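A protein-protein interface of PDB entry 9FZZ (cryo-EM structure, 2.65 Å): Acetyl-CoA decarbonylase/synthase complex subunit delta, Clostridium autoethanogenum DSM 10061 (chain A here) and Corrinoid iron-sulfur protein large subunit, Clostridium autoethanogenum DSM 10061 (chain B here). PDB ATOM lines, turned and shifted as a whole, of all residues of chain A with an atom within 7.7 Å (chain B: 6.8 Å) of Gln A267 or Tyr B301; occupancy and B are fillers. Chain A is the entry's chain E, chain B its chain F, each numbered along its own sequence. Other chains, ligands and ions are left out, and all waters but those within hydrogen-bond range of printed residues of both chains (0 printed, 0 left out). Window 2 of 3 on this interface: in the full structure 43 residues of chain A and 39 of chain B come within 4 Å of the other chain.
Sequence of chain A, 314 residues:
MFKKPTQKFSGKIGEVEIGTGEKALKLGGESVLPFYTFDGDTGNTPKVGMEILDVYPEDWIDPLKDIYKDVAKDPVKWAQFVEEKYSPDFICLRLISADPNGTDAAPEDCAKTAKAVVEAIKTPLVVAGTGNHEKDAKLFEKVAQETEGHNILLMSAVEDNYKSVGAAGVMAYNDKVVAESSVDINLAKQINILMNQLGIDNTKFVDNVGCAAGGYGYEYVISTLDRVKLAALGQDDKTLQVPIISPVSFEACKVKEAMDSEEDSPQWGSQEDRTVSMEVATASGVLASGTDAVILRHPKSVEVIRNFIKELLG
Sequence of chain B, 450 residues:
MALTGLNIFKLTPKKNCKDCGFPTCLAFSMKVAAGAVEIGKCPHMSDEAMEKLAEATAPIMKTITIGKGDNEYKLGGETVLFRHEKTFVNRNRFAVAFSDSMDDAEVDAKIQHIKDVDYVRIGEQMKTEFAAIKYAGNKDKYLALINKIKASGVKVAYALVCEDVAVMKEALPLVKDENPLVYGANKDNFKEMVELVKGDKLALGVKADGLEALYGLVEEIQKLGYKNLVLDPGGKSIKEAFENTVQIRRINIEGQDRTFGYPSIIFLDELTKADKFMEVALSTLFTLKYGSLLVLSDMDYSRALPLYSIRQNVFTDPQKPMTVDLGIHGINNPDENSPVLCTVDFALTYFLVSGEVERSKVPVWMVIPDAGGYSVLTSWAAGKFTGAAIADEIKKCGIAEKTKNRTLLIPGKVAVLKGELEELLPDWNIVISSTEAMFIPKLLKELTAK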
ATOM      1  N   LYS A 256      15.264 -17.930 -21.287  1.00  0.00           N
ATOM      2  CA  LYS A 256      14.968 -16.643 -20.671  1.00  0.00           C
ATOM      3  C   LYS A 256      14.092 -15.777 -21.563  1.00  0.00           C
ATOM      4  O   LYS A 256      13.268 -15.011 -21.058  1.00  0.00           O
ATOM      5  CB  LYS A 256      16.276 -15.923 -20.335  1.00  0.00           C
ATOM      6  CG  LYS A 256      16.084 -14.569 -19.663  1.00  0.00           C
ATOM      7  CD  LYS A 256      17.429 -13.864 -19.490  1.00  0.00           C
ATOM      8  CE  LYS A 256      17.225 -12.434 -18.982  1.00  0.00           C
ATOM      9  NZ  LYS A 256      18.525 -11.684 -18.917  1.00  0.00           N
ATOM     10  N   GLU A 257      14.254 -15.877 -22.884  1.00  0.00           N
ATOM     11  CA  GLU A 257      13.476 -15.048 -23.795  1.00  0.00           C
ATOM     12  C   GLU A 257      11.990 -15.355 -23.743  1.00  0.00           C
ATOM     13  O   GLU A 257      11.183 -14.528 -24.180  1.00  0.00           O
ATOM     14  CB  GLU A 257      13.972 -15.208 -25.237  1.00  0.00           C
ATOM     15  CG  GLU A 257      15.298 -14.500 -25.516  1.00  0.00           C
ATOM     16  CD  GLU A 257      16.487 -15.266 -24.966  1.00  0.00           C
ATOM     17  OE1 GLU A 257      16.276 -16.341 -24.378  1.00  0.00           O
ATOM     18  OE2 GLU A 257      17.632 -14.793 -25.123  1.00  0.00           O
ATOM     19  N   SER A 261       8.685 -12.704 -17.464  1.00  0.00           N
ATOM     20  CA  SER A 261       7.429 -11.983 -17.597  1.00  0.00           C
ATOM     21  C   SER A 261       7.707 -10.535 -17.981  1.00  0.00           C
ATOM     22  O   SER A 261       8.850 -10.078 -18.014  1.00  0.00           O
ATOM     23  CB  SER A 261       6.604 -12.057 -16.307  1.00  0.00           C
ATOM     24  OG  SER A 261       7.293 -11.467 -15.209  1.00  0.00           O
ATOM     25  N   GLU A 262       6.634  -9.807 -18.267  1.00  0.00           N
ATOM     26  CA  GLU A 262       6.775  -8.405 -18.629  1.00  0.00           C
ATOM     27  C   GLU A 262       7.283  -7.574 -17.463  1.00  0.00           C
ATOM     28  O   GLU A 262       7.931  -6.545 -17.677  1.00  0.00           O
ATOM     29  CB  GLU A 262       5.442  -7.862 -19.136  1.00  0.00           C
ATOM     30  CG  GLU A 262       5.566  -6.500 -19.805  1.00  0.00           C
ATOM     31  CD  GLU A 262       4.333  -6.156 -20.614  1.00  0.00           C
ATOM     32  OE1 GLU A 262       3.436  -7.015 -20.703  1.00  0.00           O
ATOM     33  OE2 GLU A 262       4.260  -5.035 -21.160  1.00  0.00           O
ATOM     34  N   GLU A 263       7.017  -8.005 -16.233  1.00  0.00           N
ATOM     35  CA  GLU A 263       7.544  -7.294 -15.074  1.00  0.00           C
ATOM     36  C   GLU A 263       9.065  -7.361 -15.033  1.00  0.00           C
ATOM     37  O   GLU A 263       9.728  -6.367 -14.719  1.00  0.00           O
ATOM     38  CB  GLU A 263       6.944  -7.867 -13.792  1.00  0.00           C
ATOM     39  CG  GLU A 263       7.357  -7.103 -12.530  1.00  0.00           C
ATOM     40  CD  GLU A 263       6.850  -7.775 -11.268  1.00  0.00           C
ATOM     41  OE1 GLU A 263       6.606  -8.994 -11.315  1.00  0.00           O
ATOM     42  OE2 GLU A 263       6.688  -7.088 -10.237  1.00  0.00           O
ATOM     43  N   ASP A 264       9.638  -8.527 -15.342  1.00  0.00           N
ATOM     44  CA  ASP A 264      11.091  -8.680 -15.324  1.00  0.00           C
ATOM     45  C   ASP A 264      11.755  -7.886 -16.442  1.00  0.00           C
ATOM     46  O   ASP A 264      12.753  -7.197 -16.210  1.00  0.00           O
ATOM     47  CB  ASP A 264      11.469 -10.155 -15.431  1.00  0.00           C
ATOM     48  CG  ASP A 264      10.785 -11.010 -14.387  1.00  0.00           C
ATOM     49  OD1 ASP A 264      10.724 -10.571 -13.220  1.00  0.00           O
ATOM     50  OD2 ASP A 264      10.297 -12.103 -14.730  1.00  0.00           O
ATOM     51  N   SER A 265      11.209  -7.954 -17.655  1.00  0.00           N
ATOM     52  CA  SER A 265      11.751  -7.249 -18.818  1.00  0.00           C
ATOM     53  C   SER A 265      10.626  -6.432 -19.435  1.00  0.00           C
ATOM     54  O   SER A 265       9.956  -6.886 -20.371  1.00  0.00           O
ATOM     55  CB  SER A 265      12.338  -8.222 -19.843  1.00  0.00           C
ATOM     56  OG  SER A 265      13.470  -8.912 -19.324  1.00  0.00           O
ATOM     57  N   PRO A 266      10.387  -5.214 -18.932  1.00  0.00           N
ATOM     58  CA  PRO A 266       9.289  -4.402 -19.490  1.00  0.00           C
ATOM     59  C   PRO A 266       9.439  -4.106 -20.969  1.00  0.00           C
ATOM     60  O   PRO A 266       8.427  -4.010 -21.674  1.00  0.00           O
ATOM     61  CB  PRO A 266       9.326  -3.120 -18.638  1.00  0.00           C
ATOM     62  CG  PRO A 266       9.987  -3.540 -17.336  1.00  0.00           C
ATOM     63  CD  PRO A 266      11.000  -4.590 -17.743  1.00  0.00           C
ATOM     64  N   GLN A 267      10.665  -3.962 -21.470  1.00  0.00           N
ATOM     65  CA  GLN A 267      10.844  -3.617 -22.875  1.00  0.00           C
ATOM     66  C   GLN A 267      10.486  -4.781 -23.794  1.00  0.00           C
ATOM     67  O   GLN A 267      10.063  -4.561 -24.932  1.00  0.00           O
ATOM     68  CB  GLN A 267      12.284  -3.148 -23.138  1.00  0.00           C
ATOM     69  CG  GLN A 267      13.362  -4.251 -23.043  1.00  0.00           C
ATOM     70  CD  GLN A 267      13.682  -4.628 -21.607  1.00  0.00           C
ATOM     71  OE1 GLN A 267      13.124  -4.059 -20.678  1.00  0.00           O
ATOM     72  NE2 GLN A 267      14.582  -5.593 -21.419  1.00  0.00           N
ATOM     73  N   TRP A 268      10.625  -6.017 -23.314  1.00  0.00           N
ATOM     74  CA  TRP A 268      10.359  -7.173 -24.162  1.00  0.00           C
ATOM     75  C   TRP A 268       8.883  -7.281 -24.523  1.00  0.00           C
ATOM     76  O   TRP A 268       8.541  -7.685 -25.641  1.00  0.00           O
ATOM     77  CB  TRP A 268      10.842  -8.444 -23.471  1.00  0.00           C
ATOM     78  CG  TRP A 268      12.320  -8.669 -23.621  1.00  0.00           C
ATOM     79  CD1 TRP A 268      13.225  -7.843 -24.230  1.00  0.00           C
ATOM     80  CD2 TRP A 268      13.064  -9.801 -23.161  1.00  0.00           C
ATOM     81  NE1 TRP A 268      14.485  -8.394 -24.172  1.00  0.00           N
ATOM     82  CE2 TRP A 268      14.408  -9.605 -23.514  1.00  0.00           C
ATOM     83  CE3 TRP A 268      12.702 -10.972 -22.471  1.00  0.00           C
ATOM     84  CZ2 TRP A 268      15.413 -10.527 -23.210  1.00  0.00           C
ATOM     85  CZ3 TRP A 268      13.702 -11.898 -22.161  1.00  0.00           C
ATOM     86  CH2 TRP A 268      15.043 -11.667 -22.536  1.00  0.00           C
ATOM     87  N   GLY A 269       7.996  -6.956 -23.592  1.00  0.00           N
ATOM     88  CA  GLY A 269       6.581  -6.959 -23.900  1.00  0.00           C
ATOM     89  C   GLY A 269       5.817  -8.154 -23.375  1.00  0.00           C
ATOM     90  O   GLY A 269       6.116  -8.663 -22.295  1.00  0.00           O
ATOM     91  N   SER A 270       4.844  -8.623 -24.153  1.00  0.00           N
ATOM     92  CA  SER A 270       3.973  -9.696 -23.701  1.00  0.00           C
ATOM     93  C   SER A 270       4.759 -10.990 -23.554  1.00  0.00           C
ATOM     94  O   SER A 270       5.514 -11.376 -24.449  1.00  0.00           O
ATOM     95  CB  SER A 270       2.821  -9.868 -24.696  1.00  0.00           C
ATOM     96  OG  SER A 270       1.897 -10.866 -24.274  1.00  0.00           O
ATOM     97  N   ASP A 273       3.291 -13.773 -25.996  1.00  0.00           N
ATOM     98  CA  ASP A 273       3.741 -13.579 -27.370  1.00  0.00           C
ATOM     99  C   ASP A 273       5.172 -14.058 -27.553  1.00  0.00           C
ATOM    100  O   ASP A 273       5.496 -14.694 -28.558  1.00  0.00           O
ATOM    101  CB  ASP A 273       3.616 -12.112 -27.767  1.00  0.00           C
ATOM    102  CG  ASP A 273       2.179 -11.685 -27.972  1.00  0.00           C
ATOM    103  OD1 ASP A 273       1.287 -12.501 -27.667  1.00  0.00           O
ATOM    104  OD2 ASP A 273       1.938 -10.557 -28.442  1.00  0.00           O
ATOM    105  N   ARG A 274       6.045 -13.759 -26.597  1.00  0.00           N
ATOM    106  CA  ARG A 274       7.428 -14.214 -26.705  1.00  0.00           C
ATOM    107  C   ARG A 274       7.517 -15.736 -26.633  1.00  0.00           C
ATOM    108  O   ARG A 274       8.300 -16.348 -27.367  1.00  0.00           O
ATOM    109  CB  ARG A 274       8.281 -13.561 -25.622  1.00  0.00           C
ATOM    110  CG  ARG A 274       8.570 -12.097 -25.932  1.00  0.00           C
ATOM    111  CD  ARG A 274       9.523 -11.494 -24.915  1.00  0.00           C
ATOM    112  NE  ARG A 274       8.837 -11.142 -23.677  1.00  0.00           N
ATOM    113  CZ  ARG A 274       8.868 -11.853 -22.556  1.00  0.00           C
ATOM    114  NH1 ARG A 274       9.559 -12.973 -22.462  1.00  0.00           N
ATOM    115  NH2 ARG A 274       8.190 -11.418 -21.494  1.00  0.00           N
ATOM    116  N   SER A 277       6.266 -17.066 -29.949  1.00  0.00           N
ATOM    117  CA  SER A 277       7.231 -16.764 -30.998  1.00  0.00           C
ATOM    118  C   SER A 277       8.436 -17.689 -30.921  1.00  0.00           C
ATOM    119  O   SER A 277       8.918 -18.176 -31.949  1.00  0.00           O
ATOM    120  CB  SER A 277       7.648 -15.296 -30.883  1.00  0.00           C
ATOM    121  OG  SER A 277       8.425 -14.878 -31.995  1.00  0.00           O
ATOM    122  N   MET A 278       8.940 -17.949 -29.715  1.00  0.00           N
ATOM    123  CA  MET A 278      10.064 -18.873 -29.571  1.00  0.00           C
ATOM    124  C   MET A 278       9.690 -20.275 -30.038  1.00  0.00           C
ATOM    125  O   MET A 278      10.446 -20.927 -30.773  1.00  0.00           O
ATOM    126  CB  MET A 278      10.525 -18.906 -28.115  1.00  0.00           C
ATOM    127  CG  MET A 278      11.315 -17.670 -27.686  1.00  0.00           C
ATOM    128  SD  MET A 278      12.912 -17.547 -28.520  1.00  0.00           S
ATOM    129  CE  MET A 278      13.650 -19.138 -28.179  1.00  0.00           C
ATOM    130  N   HIS B 113       8.822   1.641 -33.016  1.00  0.00           N
ATOM    131  CA  HIS B 113       9.162   0.226 -32.885  1.00  0.00           C
ATOM    132  C   HIS B 113      10.561  -0.063 -33.415  1.00  0.00           C
ATOM    133  O   HIS B 113      11.331  -0.799 -32.790  1.00  0.00           O
ATOM    134  CB  HIS B 113       8.132  -0.633 -33.604  1.00  0.00           C
ATOM    135  CG  HIS B 113       6.763  -0.579 -32.994  1.00  0.00           C
ATOM    136  ND1 HIS B 113       5.649  -1.066 -33.622  1.00  0.00           N
ATOM    137  CD2 HIS B 113       6.342  -0.087 -31.810  1.00  0.00           C
ATOM    138  CE1 HIS B 113       4.587  -0.876 -32.849  1.00  0.00           C
ATOM    139  NE2 HIS B 113       4.992  -0.280 -31.739  1.00  0.00           N
ATOM    140  N   ASP B 116      13.074   1.418 -30.825  1.00  0.00           N
ATOM    141  CA  ASP B 116      13.156   0.776 -29.515  1.00  0.00           C
ATOM    142  C   ASP B 116      13.785  -0.612 -29.576  1.00  0.00           C
ATOM    143  O   ASP B 116      14.534  -0.993 -28.671  1.00  0.00           O
ATOM    144  CB  ASP B 116      11.768   0.693 -28.884  1.00  0.00           C
ATOM    145  CG  ASP B 116      11.242   2.046 -28.444  1.00  0.00           C
ATOM    146  OD1 ASP B 116      12.075   2.947 -28.208  1.00  0.00           O
ATOM    147  OD2 ASP B 116      10.013   2.216 -28.335  1.00  0.00           O
ATOM    148  N   VAL B 117      13.499  -1.381 -30.623  1.00  0.00           N
ATOM    149  CA  VAL B 117      14.008  -2.745 -30.717  1.00  0.00           C
ATOM    150  C   VAL B 117      15.457  -2.692 -31.186  1.00  0.00           C
ATOM    151  O   VAL B 117      15.734  -2.684 -32.390  1.00  0.00           O
ATOM    152  CB  VAL B 117      13.151  -3.601 -31.661  1.00  0.00           C
ATOM    153  CG1 VAL B 117      13.686  -5.026 -31.712  1.00  0.00           C
ATOM    154  CG2 VAL B 117      11.705  -3.596 -31.204  1.00  0.00           C
ATOM    155  N   ASP B 118      16.382  -2.668 -30.233  1.00  0.00           N
ATOM    156  CA  ASP B 118      17.806  -2.566 -30.530  1.00  0.00           C
ATOM    157  C   ASP B 118      18.538  -3.058 -29.296  1.00  0.00           C
ATOM    158  O   ASP B 118      18.445  -2.426 -28.237  1.00  0.00           O
ATOM    159  CB  ASP B 118      18.179  -1.118 -30.856  1.00  0.00           C
ATOM    160  CG  ASP B 118      19.611  -0.967 -31.343  1.00  0.00           C
ATOM    161  OD1 ASP B 118      20.480  -1.741 -30.891  1.00  0.00           O
ATOM    162  OD2 ASP B 118      19.867  -0.079 -32.179  1.00  0.00           O
ATOM    163  N   TYR B 119      19.261  -4.167 -29.415  1.00  0.00           N
ATOM    164  CA  TYR B 119      19.969  -4.725 -28.266  1.00  0.00           C
ATOM    165  C   TYR B 119      21.272  -5.346 -28.752  1.00  0.00           C
ATOM    166  O   TYR B 119      21.633  -5.233 -29.927  1.00  0.00           O
ATOM    167  CB  TYR B 119      19.081  -5.713 -27.499  1.00  0.00           C
ATOM    168  CG  TYR B 119      18.646  -6.916 -28.292  1.00  0.00           C
ATOM    169  CD1 TYR B 119      17.542  -6.855 -29.147  1.00  0.00           C
ATOM    170  CD2 TYR B 119      19.336  -8.123 -28.188  1.00  0.00           C
ATOM    171  CE1 TYR B 119      17.141  -7.971 -29.888  1.00  0.00           C
ATOM    172  CE2 TYR B 119      18.950  -9.238 -28.914  1.00  0.00           C
ATOM    173  CZ  TYR B 119      17.858  -9.157 -29.758  1.00  0.00           C
ATOM    174  OH  TYR B 119      17.500 -10.287 -30.466  1.00  0.00           O
ATOM    175  N   MET B 299       8.139  -4.617 -36.465  1.00  0.00           N
ATOM    176  CA  MET B 299       9.265  -5.200 -35.740  1.00  0.00           C
ATOM    177  C   MET B 299       9.086  -4.930 -34.256  1.00  0.00           C
ATOM    178  O   MET B 299       9.093  -3.774 -33.833  1.00  0.00           O
ATOM    179  CB  MET B 299      10.591  -4.602 -36.240  1.00  0.00           C
ATOM    180  CG  MET B 299      11.837  -5.063 -35.467  1.00  0.00           C
ATOM    181  SD  MET B 299      12.067  -6.853 -35.511  1.00  0.00           S
ATOM    182  CE  MET B 299      12.092  -7.208 -37.265  1.00  0.00           C
ATOM    183  N   ASP B 300       8.943  -5.997 -33.464  1.00  0.00           N
ATOM    184  CA  ASP B 300       8.893  -5.890 -32.009  1.00  0.00           C
ATOM    185  C   ASP B 300       9.850  -6.900 -31.387  1.00  0.00           C
ATOM    186  O   ASP B 300      10.613  -7.556 -32.103  1.00  0.00           O
ATOM    187  CB  ASP B 300       7.473  -6.092 -31.481  1.00  0.00           C
ATOM    188  CG  ASP B 300       6.807  -7.320 -32.058  1.00  0.00           C
ATOM    189  OD1 ASP B 300       7.217  -8.441 -31.697  1.00  0.00           O
ATOM    190  OD2 ASP B 300       5.882  -7.167 -32.878  1.00  0.00           O
ATOM    191  N   TYR B 301       9.845  -7.015 -30.060  1.00  0.00           N
ATOM    192  CA  TYR B 301      10.757  -7.948 -29.406  1.00  0.00           C
ATOM    193  C   TYR B 301      10.310  -9.393 -29.570  1.00  0.00           C
ATOM    194  O   TYR B 301      11.151 -10.294 -29.635  1.00  0.00           O
ATOM    195  CB  TYR B 301      10.909  -7.603 -27.923  1.00  0.00           C
ATOM    196  CG  TYR B 301      12.005  -6.597 -27.668  1.00  0.00           C
ATOM    197  CD1 TYR B 301      13.342  -6.997 -27.595  1.00  0.00           C
ATOM    198  CD2 TYR B 301      11.712  -5.243 -27.514  1.00  0.00           C
ATOM    199  CE1 TYR B 301      14.364  -6.066 -27.367  1.00  0.00           C
ATOM    200  CE2 TYR B 301      12.717  -4.307 -27.285  1.00  0.00           C
ATOM    201  CZ  TYR B 301      14.034  -4.725 -27.213  1.00  0.00           C
ATOM    202  OH  TYR B 301      15.013  -3.775 -26.985  1.00  0.00           O
ATOM    203  N   SER B 302       9.004  -9.638 -29.662  1.00  0.00           N
ATOM    204  CA  SER B 302       8.533 -11.001 -29.885  1.00  0.00           C
ATOM    205  C   SER B 302       9.032 -11.536 -31.222  1.00  0.00           C
ATOM    206  O   SER B 302       9.363 -12.721 -31.336  1.00  0.00           O
ATOM    207  CB  SER B 302       7.007 -11.070 -29.792  1.00  0.00           C
ATOM    208  OG  SER B 302       6.388 -10.265 -30.788  1.00  0.00           O
ATOM    209  N   ARG B 303       9.087 -10.684 -32.247  1.00  0.00           N
ATOM    210  CA  ARG B 303       9.699 -11.085 -33.512  1.00  0.00           C
ATOM    211  C   ARG B 303      11.216 -11.167 -33.403  1.00  0.00           C
ATOM    212  O   ARG B 303      11.832 -12.119 -33.892  1.00  0.00           O
ATOM    213  CB  ARG B 303       9.327 -10.104 -34.623  1.00  0.00           C
ATOM    214  CG  ARG B 303       7.870 -10.141 -35.049  1.00  0.00           C
ATOM    215  CD  ARG B 303       7.668  -9.162 -36.200  1.00  0.00           C
ATOM    216  NE  ARG B 303       6.299  -9.150 -36.694  1.00  0.00           N
ATOM    217  CZ  ARG B 303       5.329  -8.385 -36.211  1.00  0.00           C
ATOM    218  NH1 ARG B 303       5.533  -7.566 -35.195  1.00  0.00           N
ATOM    219  NH2 ARG B 303       4.117  -8.445 -36.761  1.00  0.00           N
ATOM    220  N   ALA B 304      11.835 -10.171 -32.776  1.00  0.00           N
ATOM    221  CA  ALA B 304      13.281 -10.005 -32.872  1.00  0.00           C
ATOM    222  C   ALA B 304      14.025 -11.057 -32.062  1.00  0.00           C
ATOM    223  O   ALA B 304      15.066 -11.558 -32.499  1.00  0.00           O
ATOM    224  CB  ALA B 304      13.677  -8.598 -32.421  1.00  0.00           C
ATOM    225  N   LEU B 305      13.522 -11.401 -30.881  1.00  0.00           N
ATOM    226  CA  LEU B 305      14.267 -12.301 -30.002  1.00  0.00           C
ATOM    227  C   LEU B 305      14.541 -13.654 -30.642  1.00  0.00           C
ATOM    228  O   LEU B 305      15.698 -14.109 -30.593  1.00  0.00           O
ATOM    229  CB  LEU B 305      13.539 -12.451 -28.662  1.00  0.00           C
ATOM    230  CG  LEU B 305      13.620 -11.218 -27.747  1.00  0.00           C
ATOM    231  CD1 LEU B 305      12.759 -11.421 -26.516  1.00  0.00           C
ATOM    232  CD2 LEU B 305      15.063 -10.917 -27.346  1.00  0.00           C
ATOM    233  N   PRO B 306      13.570 -14.349 -31.239  1.00  0.00           N
ATOM    234  CA  PRO B 306      13.915 -15.631 -31.881  1.00  0.00           C
ATOM    235  C   PRO B 306      14.659 -15.464 -33.190  1.00  0.00           C
ATOM    236  O   PRO B 306      15.622 -16.197 -33.450  1.00  0.00           O
ATOM    237  CB  PRO B 306      12.550 -16.313 -32.080  1.00  0.00           C
ATOM    238  CG  PRO B 306      11.562 -15.497 -31.263  1.00  0.00           C
ATOM    239  CD  PRO B 306      12.118 -14.111 -31.247  1.00  0.00           C
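OG of Ser A277 is in hydrogen-bond range of O of Ser B302 (2.4 Å).
The backbone carbonyl oxygen (O) of Glu A257 sits at hydrogen-bond distance from the guanidinium group (NH1) of Arg A274, at 2.8 Å.
The backbone carbonyl oxygen (O) of Ser A270 lies within hydrogen-bond range of the guanidinium group (NE) of Arg A274 (3.4 Å).
O of Asp B116 sits at hydrogen-bond distance from OH of Tyr B301 (3.3 Å).
The side-chain carboxylate of Asp B300 lies within hydrogen-bond range of the backbone NH of Ser B302 (3.0 Å).
Among the printed residues, merely in contact across the chains: Gln A267 with Tyr B301 (3.1 Å), Trp A268 with Tyr B301 (3.3 Å), Trp A268 with Leu B305 (3.7 Å), Arg A274 with Leu B305 (3.6 Å), Ser A277 with Pro B306 (3.3 Å) and Met A278 with Pro B306 (3.7 Å).
Of chain B, only Tyr B301 comes within 4 Å of Gln A267.
Of the printed residues of chain B, Trp A268 touches Tyr B301 (3.3 Å) and Leu B305 (3.7 Å).
Asp A273 touches none of the printed residues of chain B.
Of the printed residues of chain B, Ser A277 touches Ser B302 and Pro B306.
Of the printed residues of chain B, Met A278 touches Pro B306 (3.7 Å).
Tyr B301 touches just these residues of chain A: Gln A267 and Trp A268.
Of the printed residues of chain A, Ser B302 touches Ser A277.
Of the printed residues of chain A, Leu B305 touches Trp A268 and Arg A274.
The nearest residue of chain A that does not touch Tyr B301 is Arg A274 (4.9 Å).
Along chain B the printed residues that touch a printed residue of chain A span positions 301 to 306.
Printed residues of chain A that touch a printed residue of chain B: Gln A267, Trp A268, Arg A274, Ser A277 and Met A278.
Among the printed residues, 7 pairs touch across the chains.
Among the printed residues, no Asp or Glu carboxylate lies within 4 Å of a Lys or Arg side-chain nitrogen of the other chain.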
